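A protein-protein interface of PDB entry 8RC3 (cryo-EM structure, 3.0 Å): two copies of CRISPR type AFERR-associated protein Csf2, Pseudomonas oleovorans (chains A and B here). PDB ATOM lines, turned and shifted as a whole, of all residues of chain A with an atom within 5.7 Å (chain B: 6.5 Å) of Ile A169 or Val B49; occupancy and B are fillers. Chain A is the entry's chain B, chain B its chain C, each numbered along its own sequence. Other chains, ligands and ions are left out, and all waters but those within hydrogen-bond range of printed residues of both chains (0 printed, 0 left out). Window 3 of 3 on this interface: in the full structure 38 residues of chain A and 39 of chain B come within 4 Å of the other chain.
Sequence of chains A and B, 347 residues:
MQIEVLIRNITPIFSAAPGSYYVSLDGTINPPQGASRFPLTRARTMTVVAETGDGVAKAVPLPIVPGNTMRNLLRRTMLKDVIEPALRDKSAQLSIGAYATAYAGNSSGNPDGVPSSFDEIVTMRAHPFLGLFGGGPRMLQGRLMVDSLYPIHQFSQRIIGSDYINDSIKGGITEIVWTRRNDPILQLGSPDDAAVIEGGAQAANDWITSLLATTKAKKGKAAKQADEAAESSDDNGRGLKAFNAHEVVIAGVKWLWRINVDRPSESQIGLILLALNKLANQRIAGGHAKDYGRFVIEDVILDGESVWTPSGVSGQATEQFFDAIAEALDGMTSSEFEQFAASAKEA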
ATOM      1  N   ILE A 152      -5.139  13.238 -10.783  1.00  0.00           N
ATOM      2  CA  ILE A 152      -6.355  13.231  -9.985  1.00  0.00           C
ATOM      3  C   ILE A 152      -6.542  14.637  -9.444  1.00  0.00           C
ATOM      4  O   ILE A 152      -5.874  15.050  -8.489  1.00  0.00           O
ATOM      5  CB  ILE A 152      -6.303  12.188  -8.863  1.00  0.00           C
ATOM      6  CG1 ILE A 152      -6.101  10.798  -9.456  1.00  0.00           C
ATOM      7  CG2 ILE A 152      -7.576  12.228  -8.053  1.00  0.00           C
ATOM      8  CD1 ILE A 152      -6.100   9.716  -8.428  1.00  0.00           C
ATOM      9  N   HIS A 153      -7.454  15.377 -10.062  1.00  0.00           N
ATOM     10  CA  HIS A 153      -7.595  16.806  -9.864  1.00  0.00           C
ATOM     11  C   HIS A 153      -9.076  17.131  -9.793  1.00  0.00           C
ATOM     12  O   HIS A 153      -9.930  16.308 -10.131  1.00  0.00           O
ATOM     13  CB  HIS A 153      -6.916  17.576 -11.003  1.00  0.00           C
ATOM     14  CG  HIS A 153      -6.544  18.983 -10.660  1.00  0.00           C
ATOM     15  ND1 HIS A 153      -7.405  20.042 -10.840  1.00  0.00           N
ATOM     16  CD2 HIS A 153      -5.396  19.508 -10.176  1.00  0.00           C
ATOM     17  CE1 HIS A 153      -6.808  21.159 -10.466  1.00  0.00           C
ATOM     18  NE2 HIS A 153      -5.587  20.864 -10.061  1.00  0.00           N
ATOM     19  N   GLN A 154      -9.384  18.346  -9.342  1.00  0.00           N
ATOM     20  CA  GLN A 154     -10.763  18.810  -9.407  1.00  0.00           C
ATOM     21  C   GLN A 154     -11.228  18.957 -10.847  1.00  0.00           C
ATOM     22  O   GLN A 154     -12.420  18.808 -11.134  1.00  0.00           O
ATOM     23  CB  GLN A 154     -10.905  20.135  -8.665  1.00  0.00           C
ATOM     24  CG  GLN A 154     -12.337  20.591  -8.486  1.00  0.00           C
ATOM     25  CD  GLN A 154     -12.429  21.989  -7.922  1.00  0.00           C
ATOM     26  OE1 GLN A 154     -11.577  22.835  -8.189  1.00  0.00           O
ATOM     27  NE2 GLN A 154     -13.465  22.240  -7.132  1.00  0.00           N
ATOM     28  N   ASP A 167      -7.850  11.567  -3.307  1.00  0.00           N
ATOM     29  CA  ASP A 167      -6.530  11.945  -3.788  1.00  0.00           C
ATOM     30  C   ASP A 167      -6.544  13.242  -4.584  1.00  0.00           C
ATOM     31  O   ASP A 167      -5.490  13.667  -5.065  1.00  0.00           O
ATOM     32  CB  ASP A 167      -5.944  10.823  -4.647  1.00  0.00           C
ATOM     33  CG  ASP A 167      -5.790   9.527  -3.883  1.00  0.00           C
ATOM     34  OD1 ASP A 167      -5.638   9.580  -2.644  1.00  0.00           O
ATOM     35  OD2 ASP A 167      -5.818   8.453  -4.519  1.00  0.00           O
ATOM     36  N   SER A 168      -7.704  13.873  -4.733  1.00  0.00           N
ATOM     37  CA  SER A 168      -7.818  15.074  -5.543  1.00  0.00           C
ATOM     38  C   SER A 168      -7.055  16.234  -4.914  1.00  0.00           C
ATOM     39  O   SER A 168      -6.979  16.370  -3.691  1.00  0.00           O
ATOM     40  CB  SER A 168      -9.286  15.454  -5.724  1.00  0.00           C
ATOM     41  OG  SER A 168      -9.428  16.527  -6.634  1.00  0.00           O
ATOM     42  N   ILE A 169      -6.483  17.073  -5.772  1.00  0.00           N
ATOM     43  CA  ILE A 169      -5.768  18.275  -5.365  1.00  0.00           C
ATOM     44  C   ILE A 169      -6.442  19.468  -6.030  1.00  0.00           C
ATOM     45  O   ILE A 169      -6.715  19.441  -7.235  1.00  0.00           O
ATOM     46  CB  ILE A 169      -4.273  18.193  -5.725  1.00  0.00           C
ATOM     47  CG1 ILE A 169      -3.580  19.533  -5.476  1.00  0.00           C
ATOM     48  CG2 ILE A 169      -4.086  17.725  -7.157  1.00  0.00           C
ATOM     49  CD1 ILE A 169      -2.073  19.444  -5.483  1.00  0.00           C
ATOM     50  N   LYS A 170      -6.716  20.506  -5.242  1.00  0.00           N
ATOM     51  CA  LYS A 170      -7.602  21.578  -5.685  1.00  0.00           C
ATOM     52  C   LYS A 170      -6.897  22.558  -6.615  1.00  0.00           C
ATOM     53  O   LYS A 170      -7.292  22.727  -7.774  1.00  0.00           O
ATOM     54  CB  LYS A 170      -8.170  22.312  -4.470  1.00  0.00           C
ATOM     55  CG  LYS A 170      -9.063  21.455  -3.588  1.00  0.00           C
ATOM     56  CD  LYS A 170     -10.406  21.191  -4.247  1.00  0.00           C
ATOM     57  CE  LYS A 170     -11.026  22.474  -4.774  1.00  0.00           C
ATOM     58  NZ  LYS A 170     -11.086  23.536  -3.731  1.00  0.00           N
ATOM     59  N   GLY A 171      -5.853  23.215  -6.125  1.00  0.00           N
ATOM     60  CA  GLY A 171      -5.252  24.325  -6.831  1.00  0.00           C
ATOM     61  C   GLY A 171      -4.406  23.889  -8.009  1.00  0.00           C
ATOM     62  O   GLY A 171      -4.391  22.729  -8.423  1.00  0.00           O
ATOM     63  N   GLY A 172      -3.695  24.866  -8.568  1.00  0.00           N
ATOM     64  CA  GLY A 172      -2.798  24.572  -9.671  1.00  0.00           C
ATOM     65  C   GLY A 172      -1.687  23.629  -9.244  1.00  0.00           C
ATOM     66  O   GLY A 172      -1.141  23.734  -8.144  1.00  0.00           O
ATOM     67  N   ILE A 173      -1.350  22.701 -10.133  1.00  0.00           N
ATOM     68  CA  ILE A 173      -0.343  21.687  -9.871  1.00  0.00           C
ATOM     69  C   ILE A 173       0.883  21.886 -10.757  1.00  0.00           C
ATOM     70  O   ILE A 173       1.699  20.982 -10.902  1.00  0.00           O
ATOM     71  CB  ILE A 173      -0.925  20.277 -10.039  1.00  0.00           C
ATOM     72  CG1 ILE A 173      -1.432  20.086 -11.465  1.00  0.00           C
ATOM     73  CG2 ILE A 173      -2.064  20.068  -9.077  1.00  0.00           C
ATOM     74  CD1 ILE A 173      -1.981  18.712 -11.731  1.00  0.00           C
ATOM     75  N   ILE A 250       4.155  19.828 -10.583  1.00  0.00           N
ATOM     76  CA  ILE A 250       4.819  19.728  -9.293  1.00  0.00           C
ATOM     77  C   ILE A 250       4.907  18.272  -8.848  1.00  0.00           C
ATOM     78  O   ILE A 250       4.148  17.402  -9.291  1.00  0.00           O
ATOM     79  CB  ILE A 250       4.101  20.582  -8.237  1.00  0.00           C
ATOM     80  CG1 ILE A 250       2.709  20.035  -7.942  1.00  0.00           C
ATOM     81  CG2 ILE A 250       3.997  22.015  -8.701  1.00  0.00           C
ATOM     82  CD1 ILE A 250       1.917  20.913  -7.009  1.00  0.00           C
ATOM     83  N   ALA A 251       5.860  18.009  -7.962  1.00  0.00           N
ATOM     84  CA  ALA A 251       6.125  16.659  -7.496  1.00  0.00           C
ATOM     85  C   ALA A 251       5.177  16.276  -6.372  1.00  0.00           C
ATOM     86  O   ALA A 251       4.869  17.087  -5.497  1.00  0.00           O
ATOM     87  CB  ALA A 251       7.573  16.544  -7.025  1.00  0.00           C
ATOM     88  N   GLY A 252       4.721  15.026  -6.395  1.00  0.00           N
ATOM     89  CA  GLY A 252       3.843  14.503  -5.372  1.00  0.00           C
ATOM     90  C   GLY A 252       2.380  14.419  -5.745  1.00  0.00           C
ATOM     91  O   GLY A 252       1.567  14.031  -4.897  1.00  0.00           O
ATOM     92  N   VAL A 253       2.017  14.763  -6.971  1.00  0.00           N
ATOM     93  CA  VAL A 253       0.629  14.727  -7.417  1.00  0.00           C
ATOM     94  C   VAL A 253       0.309  13.330  -7.933  1.00  0.00           C
ATOM     95  O   VAL A 253       1.156  12.668  -8.541  1.00  0.00           O
ATOM     96  CB  VAL A 253       0.370  15.807  -8.485  1.00  0.00           C
ATOM     97  CG1 VAL A 253       1.166  15.534  -9.735  1.00  0.00           C
ATOM     98  CG2 VAL A 253      -1.108  15.898  -8.809  1.00  0.00           C
ATOM     99  N   THR B  47       7.191  24.392  -5.716  1.00  0.00           N
ATOM    100  CA  THR B  47       5.932  23.922  -5.160  1.00  0.00           C
ATOM    101  C   THR B  47       5.892  22.402  -5.178  1.00  0.00           C
ATOM    102  O   THR B  47       6.213  21.773  -6.189  1.00  0.00           O
ATOM    103  CB  THR B  47       4.760  24.492  -5.953  1.00  0.00           C
ATOM    104  OG1 THR B  47       4.855  25.920  -5.990  1.00  0.00           O
ATOM    105  CG2 THR B  47       3.445  24.099  -5.311  1.00  0.00           C
ATOM    106  N   VAL B  48       5.520  21.811  -4.047  1.00  0.00           N
ATOM    107  CA  VAL B  48       5.394  20.366  -3.927  1.00  0.00           C
ATOM    108  C   VAL B  48       4.105  20.050  -3.189  1.00  0.00           C
ATOM    109  O   VAL B  48       3.608  20.854  -2.395  1.00  0.00           O
ATOM    110  CB  VAL B  48       6.596  19.729  -3.197  1.00  0.00           C
ATOM    111  CG1 VAL B  48       7.853  19.858  -4.034  1.00  0.00           C
ATOM    112  CG2 VAL B  48       6.789  20.367  -1.839  1.00  0.00           C
ATOM    113  N   VAL B  49       3.563  18.873  -3.460  1.00  0.00           N
ATOM    114  CA  VAL B  49       2.384  18.383  -2.764  1.00  0.00           C
ATOM    115  C   VAL B  49       2.835  17.732  -1.466  1.00  0.00           C
ATOM    116  O   VAL B  49       3.761  16.913  -1.462  1.00  0.00           O
ATOM    117  CB  VAL B  49       1.600  17.394  -3.638  1.00  0.00           C
ATOM    118  CG1 VAL B  49       0.299  17.024  -2.970  1.00  0.00           C
ATOM    119  CG2 VAL B  49       1.337  17.995  -4.998  1.00  0.00           C
ATOM    120  N   ALA B  50       2.200  18.106  -0.361  1.00  0.00           N
ATOM    121  CA  ALA B  50       2.581  17.597   0.944  1.00  0.00           C
ATOM    122  C   ALA B  50       1.341  17.405   1.801  1.00  0.00           C
ATOM    123  O   ALA B  50       0.360  18.141   1.674  1.00  0.00           O
ATOM    124  CB  ALA B  50       3.559  18.538   1.650  1.00  0.00           C
ATOM    125  N   GLU B  51       1.397  16.409   2.677  1.00  0.00           N
ATOM    126  CA  GLU B  51       0.334  16.166   3.641  1.00  0.00           C
ATOM    127  C   GLU B  51       0.653  16.932   4.918  1.00  0.00           C
ATOM    128  O   GLU B  51       1.699  16.710   5.537  1.00  0.00           O
ATOM    129  CB  GLU B  51       0.184  14.673   3.929  1.00  0.00           C
ATOM    130  CG  GLU B  51      -0.182  13.838   2.713  1.00  0.00           C
ATOM    131  CD  GLU B  51       1.033  13.299   1.985  1.00  0.00           C
ATOM    132  OE1 GLU B  51       2.160  13.731   2.308  1.00  0.00           O
ATOM    133  OE2 GLU B  51       0.861  12.442   1.093  1.00  0.00           O
ATOM    134  N   ALA B  57      -3.874  16.447   0.804  1.00  0.00           N
ATOM    135  CA  ALA B  57      -2.763  16.881  -0.029  1.00  0.00           C
ATOM    136  C   ALA B  57      -2.833  18.386  -0.254  1.00  0.00           C
ATOM    137  O   ALA B  57      -3.885  18.919  -0.617  1.00  0.00           O
ATOM    138  CB  ALA B  57      -2.785  16.144  -1.366  1.00  0.00           C
ATOM    139  N   LYS B  58      -1.712  19.066  -0.036  1.00  0.00           N
ATOM    140  CA  LYS B  58      -1.622  20.508  -0.206  1.00  0.00           C
ATOM    141  C   LYS B  58      -0.362  20.857  -0.980  1.00  0.00           C
ATOM    142  O   LYS B  58       0.692  20.252  -0.770  1.00  0.00           O
ATOM    143  CB  LYS B  58      -1.610  21.229   1.143  1.00  0.00           C
ATOM    144  CG  LYS B  58      -2.986  21.550   1.688  1.00  0.00           C
ATOM    145  CD  LYS B  58      -2.920  22.694   2.680  1.00  0.00           C
ATOM    146  CE  LYS B  58      -2.440  23.971   2.014  1.00  0.00           C
ATOM    147  NZ  LYS B  58      -3.088  24.182   0.690  1.00  0.00           N
ATOM    148  N   ALA B  59      -0.475  21.837  -1.870  1.00  0.00           N
ATOM    149  CA  ALA B  59       0.669  22.347  -2.614  1.00  0.00           C
ATOM    150  C   ALA B  59       1.309  23.460  -1.795  1.00  0.00           C
ATOM    151  O   ALA B  59       0.709  24.521  -1.600  1.00  0.00           O
ATOM    152  CB  ALA B  59       0.245  22.844  -3.991  1.00  0.00           C
ATOM    153  N   VAL B  60       2.525  23.218  -1.317  1.00  0.00           N
ATOM    154  CA  VAL B  60       3.218  24.162  -0.448  1.00  0.00           C
ATOM    155  C   VAL B  60       4.584  24.470  -1.045  1.00  0.00           C
ATOM    156  O   VAL B  60       5.159  23.621  -1.739  1.00  0.00           O
ATOM    157  CB  VAL B  60       3.351  23.606   0.978  1.00  0.00           C
ATOM    158  CG1 VAL B  60       1.998  23.562   1.657  1.00  0.00           C
ATOM    159  CG2 VAL B  60       3.969  22.223   0.945  1.00  0.00           C
ATOM    160  N   PHE B 155       7.370  18.973   4.648  1.00  0.00           N
ATOM    161  CA  PHE B 155       6.752  19.204   3.351  1.00  0.00           C
ATOM    162  C   PHE B 155       7.364  18.376   2.233  1.00  0.00           C
ATOM    163  O   PHE B 155       6.866  18.431   1.104  1.00  0.00           O
ATOM    164  CB  PHE B 155       6.843  20.686   2.978  1.00  0.00           C
ATOM    165  CG  PHE B 155       6.008  21.583   3.843  1.00  0.00           C
ATOM    166  CD1 PHE B 155       5.003  21.064   4.638  1.00  0.00           C
ATOM    167  CD2 PHE B 155       6.229  22.948   3.859  1.00  0.00           C
ATOM    168  CE1 PHE B 155       4.235  21.887   5.431  1.00  0.00           C
ATOM    169  CE2 PHE B 155       5.462  23.775   4.651  1.00  0.00           C
ATOM    170  CZ  PHE B 155       4.465  23.243   5.439  1.00  0.00           C
ATOM    171  N   SER B 156       8.426  17.621   2.504  1.00  0.00           N
ATOM    172  CA  SER B 156       9.088  16.830   1.476  1.00  0.00           C
ATOM    173  C   SER B 156       9.016  15.334   1.744  1.00  0.00           C
ATOM    174  O   SER B 156       9.683  14.561   1.048  1.00  0.00           O
ATOM    175  CB  SER B 156      10.548  17.262   1.328  1.00  0.00           C
ATOM    176  OG  SER B 156      11.212  17.238   2.576  1.00  0.00           O
ATOM    177  N   GLN B 157       8.226  14.901   2.729  1.00  0.00           N
ATOM    178  CA  GLN B 157       8.108  13.474   3.001  1.00  0.00           C
ATOM    179  C   GLN B 157       7.400  12.743   1.868  1.00  0.00           C
ATOM    180  O   GLN B 157       7.709  11.579   1.593  1.00  0.00           O
ATOM    181  CB  GLN B 157       7.374  13.251   4.320  1.00  0.00           C
ATOM    182  CG  GLN B 157       8.083  13.850   5.518  1.00  0.00           C
ATOM    183  CD  GLN B 157       9.436  13.217   5.773  1.00  0.00           C
ATOM    184  OE1 GLN B 157       9.659  12.052   5.450  1.00  0.00           O
ATOM    185  NE2 GLN B 157      10.348  13.986   6.354  1.00  0.00           N
ATOM    186  N   ARG B 158       6.456  13.406   1.203  1.00  0.00           N
ATOM    187  CA  ARG B 158       5.785  12.838   0.042  1.00  0.00           C
ATOM    188  C   ARG B 158       6.718  12.670  -1.148  1.00  0.00           C
ATOM    189  O   ARG B 158       6.358  11.976  -2.105  1.00  0.00           O
ATOM    190  CB  ARG B 158       4.600  13.725  -0.340  1.00  0.00           C
ATOM    191  CG  ARG B 158       3.545  13.075  -1.211  1.00  0.00           C
ATOM    192  CD  ARG B 158       2.416  14.052  -1.464  1.00  0.00           C
ATOM    193  NE  ARG B 158       1.476  13.599  -2.480  1.00  0.00           N
ATOM    194  CZ  ARG B 158       0.292  13.065  -2.218  1.00  0.00           C
ATOM    195  NH1 ARG B 158      -0.114  12.863  -0.976  1.00  0.00           N
ATOM    196  NH2 ARG B 158      -0.507  12.732  -3.226  1.00  0.00           N
ATOM    197  N   ILE B 159       7.899  13.282  -1.114  1.00  0.00           N
ATOM    198  CA  ILE B 159       8.857  13.226  -2.216  1.00  0.00           C
ATOM    199  C   ILE B 159      10.063  12.365  -1.854  1.00  0.00           C
ATOM    200  O   ILE B 159      10.341  11.363  -2.511  1.00  0.00           O
ATOM    201  CB  ILE B 159       9.290  14.645  -2.644  1.00  0.00           C
ATOM    202  CG1 ILE B 159       8.100  15.412  -3.212  1.00  0.00           C
ATOM    203  CG2 ILE B 159      10.411  14.576  -3.654  1.00  0.00           C
ATOM    204  CD1 ILE B 159       7.178  14.564  -4.050  1.00  0.00           C
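Val B49 touches just these residues of chain A: Ile A169 (3.7 Å), Ile A250 (3.6 Å), Ala A251 (3.0 Å), Gly A252 (3.6 Å) and Val A253 (3.8 Å).
Of the printed residues of chain A, Ile B159 touches Ala A251 and Gly A252.
Printed residues of chain B within 4 Å of Val A253: Val B49.
Of the printed residues of chain B, Gly A252 touches Val B49, Arg B158 and Ile B159.
Printed residues of chain A within 4 Å of Ala B59: Ile A250 (3.95 Å).
The nearest printed residue of chain A that does not touch Val B49 is Ile A173 (5.7 Å).
No position is printed for both chains.
Of the 11 pairs that touch across the chains among the printed residues, none has its exchanged pair printed and touching as well.
Among the printed residues, pairs that only touch across the chains: Ile A169 with Val B49, Ile A250 with Thr B47, Ile A250 with Val B49, Ile A250 with Ala B59, Ala A251 with Val B48, Ala A251 with Ile B159, Gly A252 with Val B49, Gly A252 with Ile B159 and Val A253 with Val B49.
Printed residues of chain B that touch a printed residue of chain A: Thr B47, Val B48, Val B49, Ala B59, Arg B158 and Ile B159.
Hydrophobic or aromatic side chains of chain B within 4 Å of the printed part of chain A: Val B48, Val B49, Ala B59 and Ile B159.
Printed residues of chain A that touch a printed residue of chain B: Ile A169, Ile A250, Ala A251, Gly A252 and Val A253.
The backbone carbonyl oxygen of Ala A251 sits at hydrogen-bond distance from the backbone NH of Val B49 (3.0 Å).
The guanidinium group (NE) of Arg B158 is in hydrogen-bond range of the backbone carbonyl oxygen (O) of Gly A252, at 2.5 Å.
The backbone NH of Ile A169 lies within hydrogen-bond range of the backbone carbonyl oxygen of Ile A152.
A ring nitrogen (NE2) of His A153 lies close to the backbone carbonyl oxygen (O) of Ile A169, 3.4 Å away.
The backbone carbonyl oxygen of Ile A173 is in hydrogen-bond range of the backbone NH of Ile A250.
O of Val B48 lies within hydrogen-bond range of N of Val B60, 2.8 Å away.
OE2 of Glu B51 is in salt-bridge range of NE of Arg B158 (3.8 Å).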
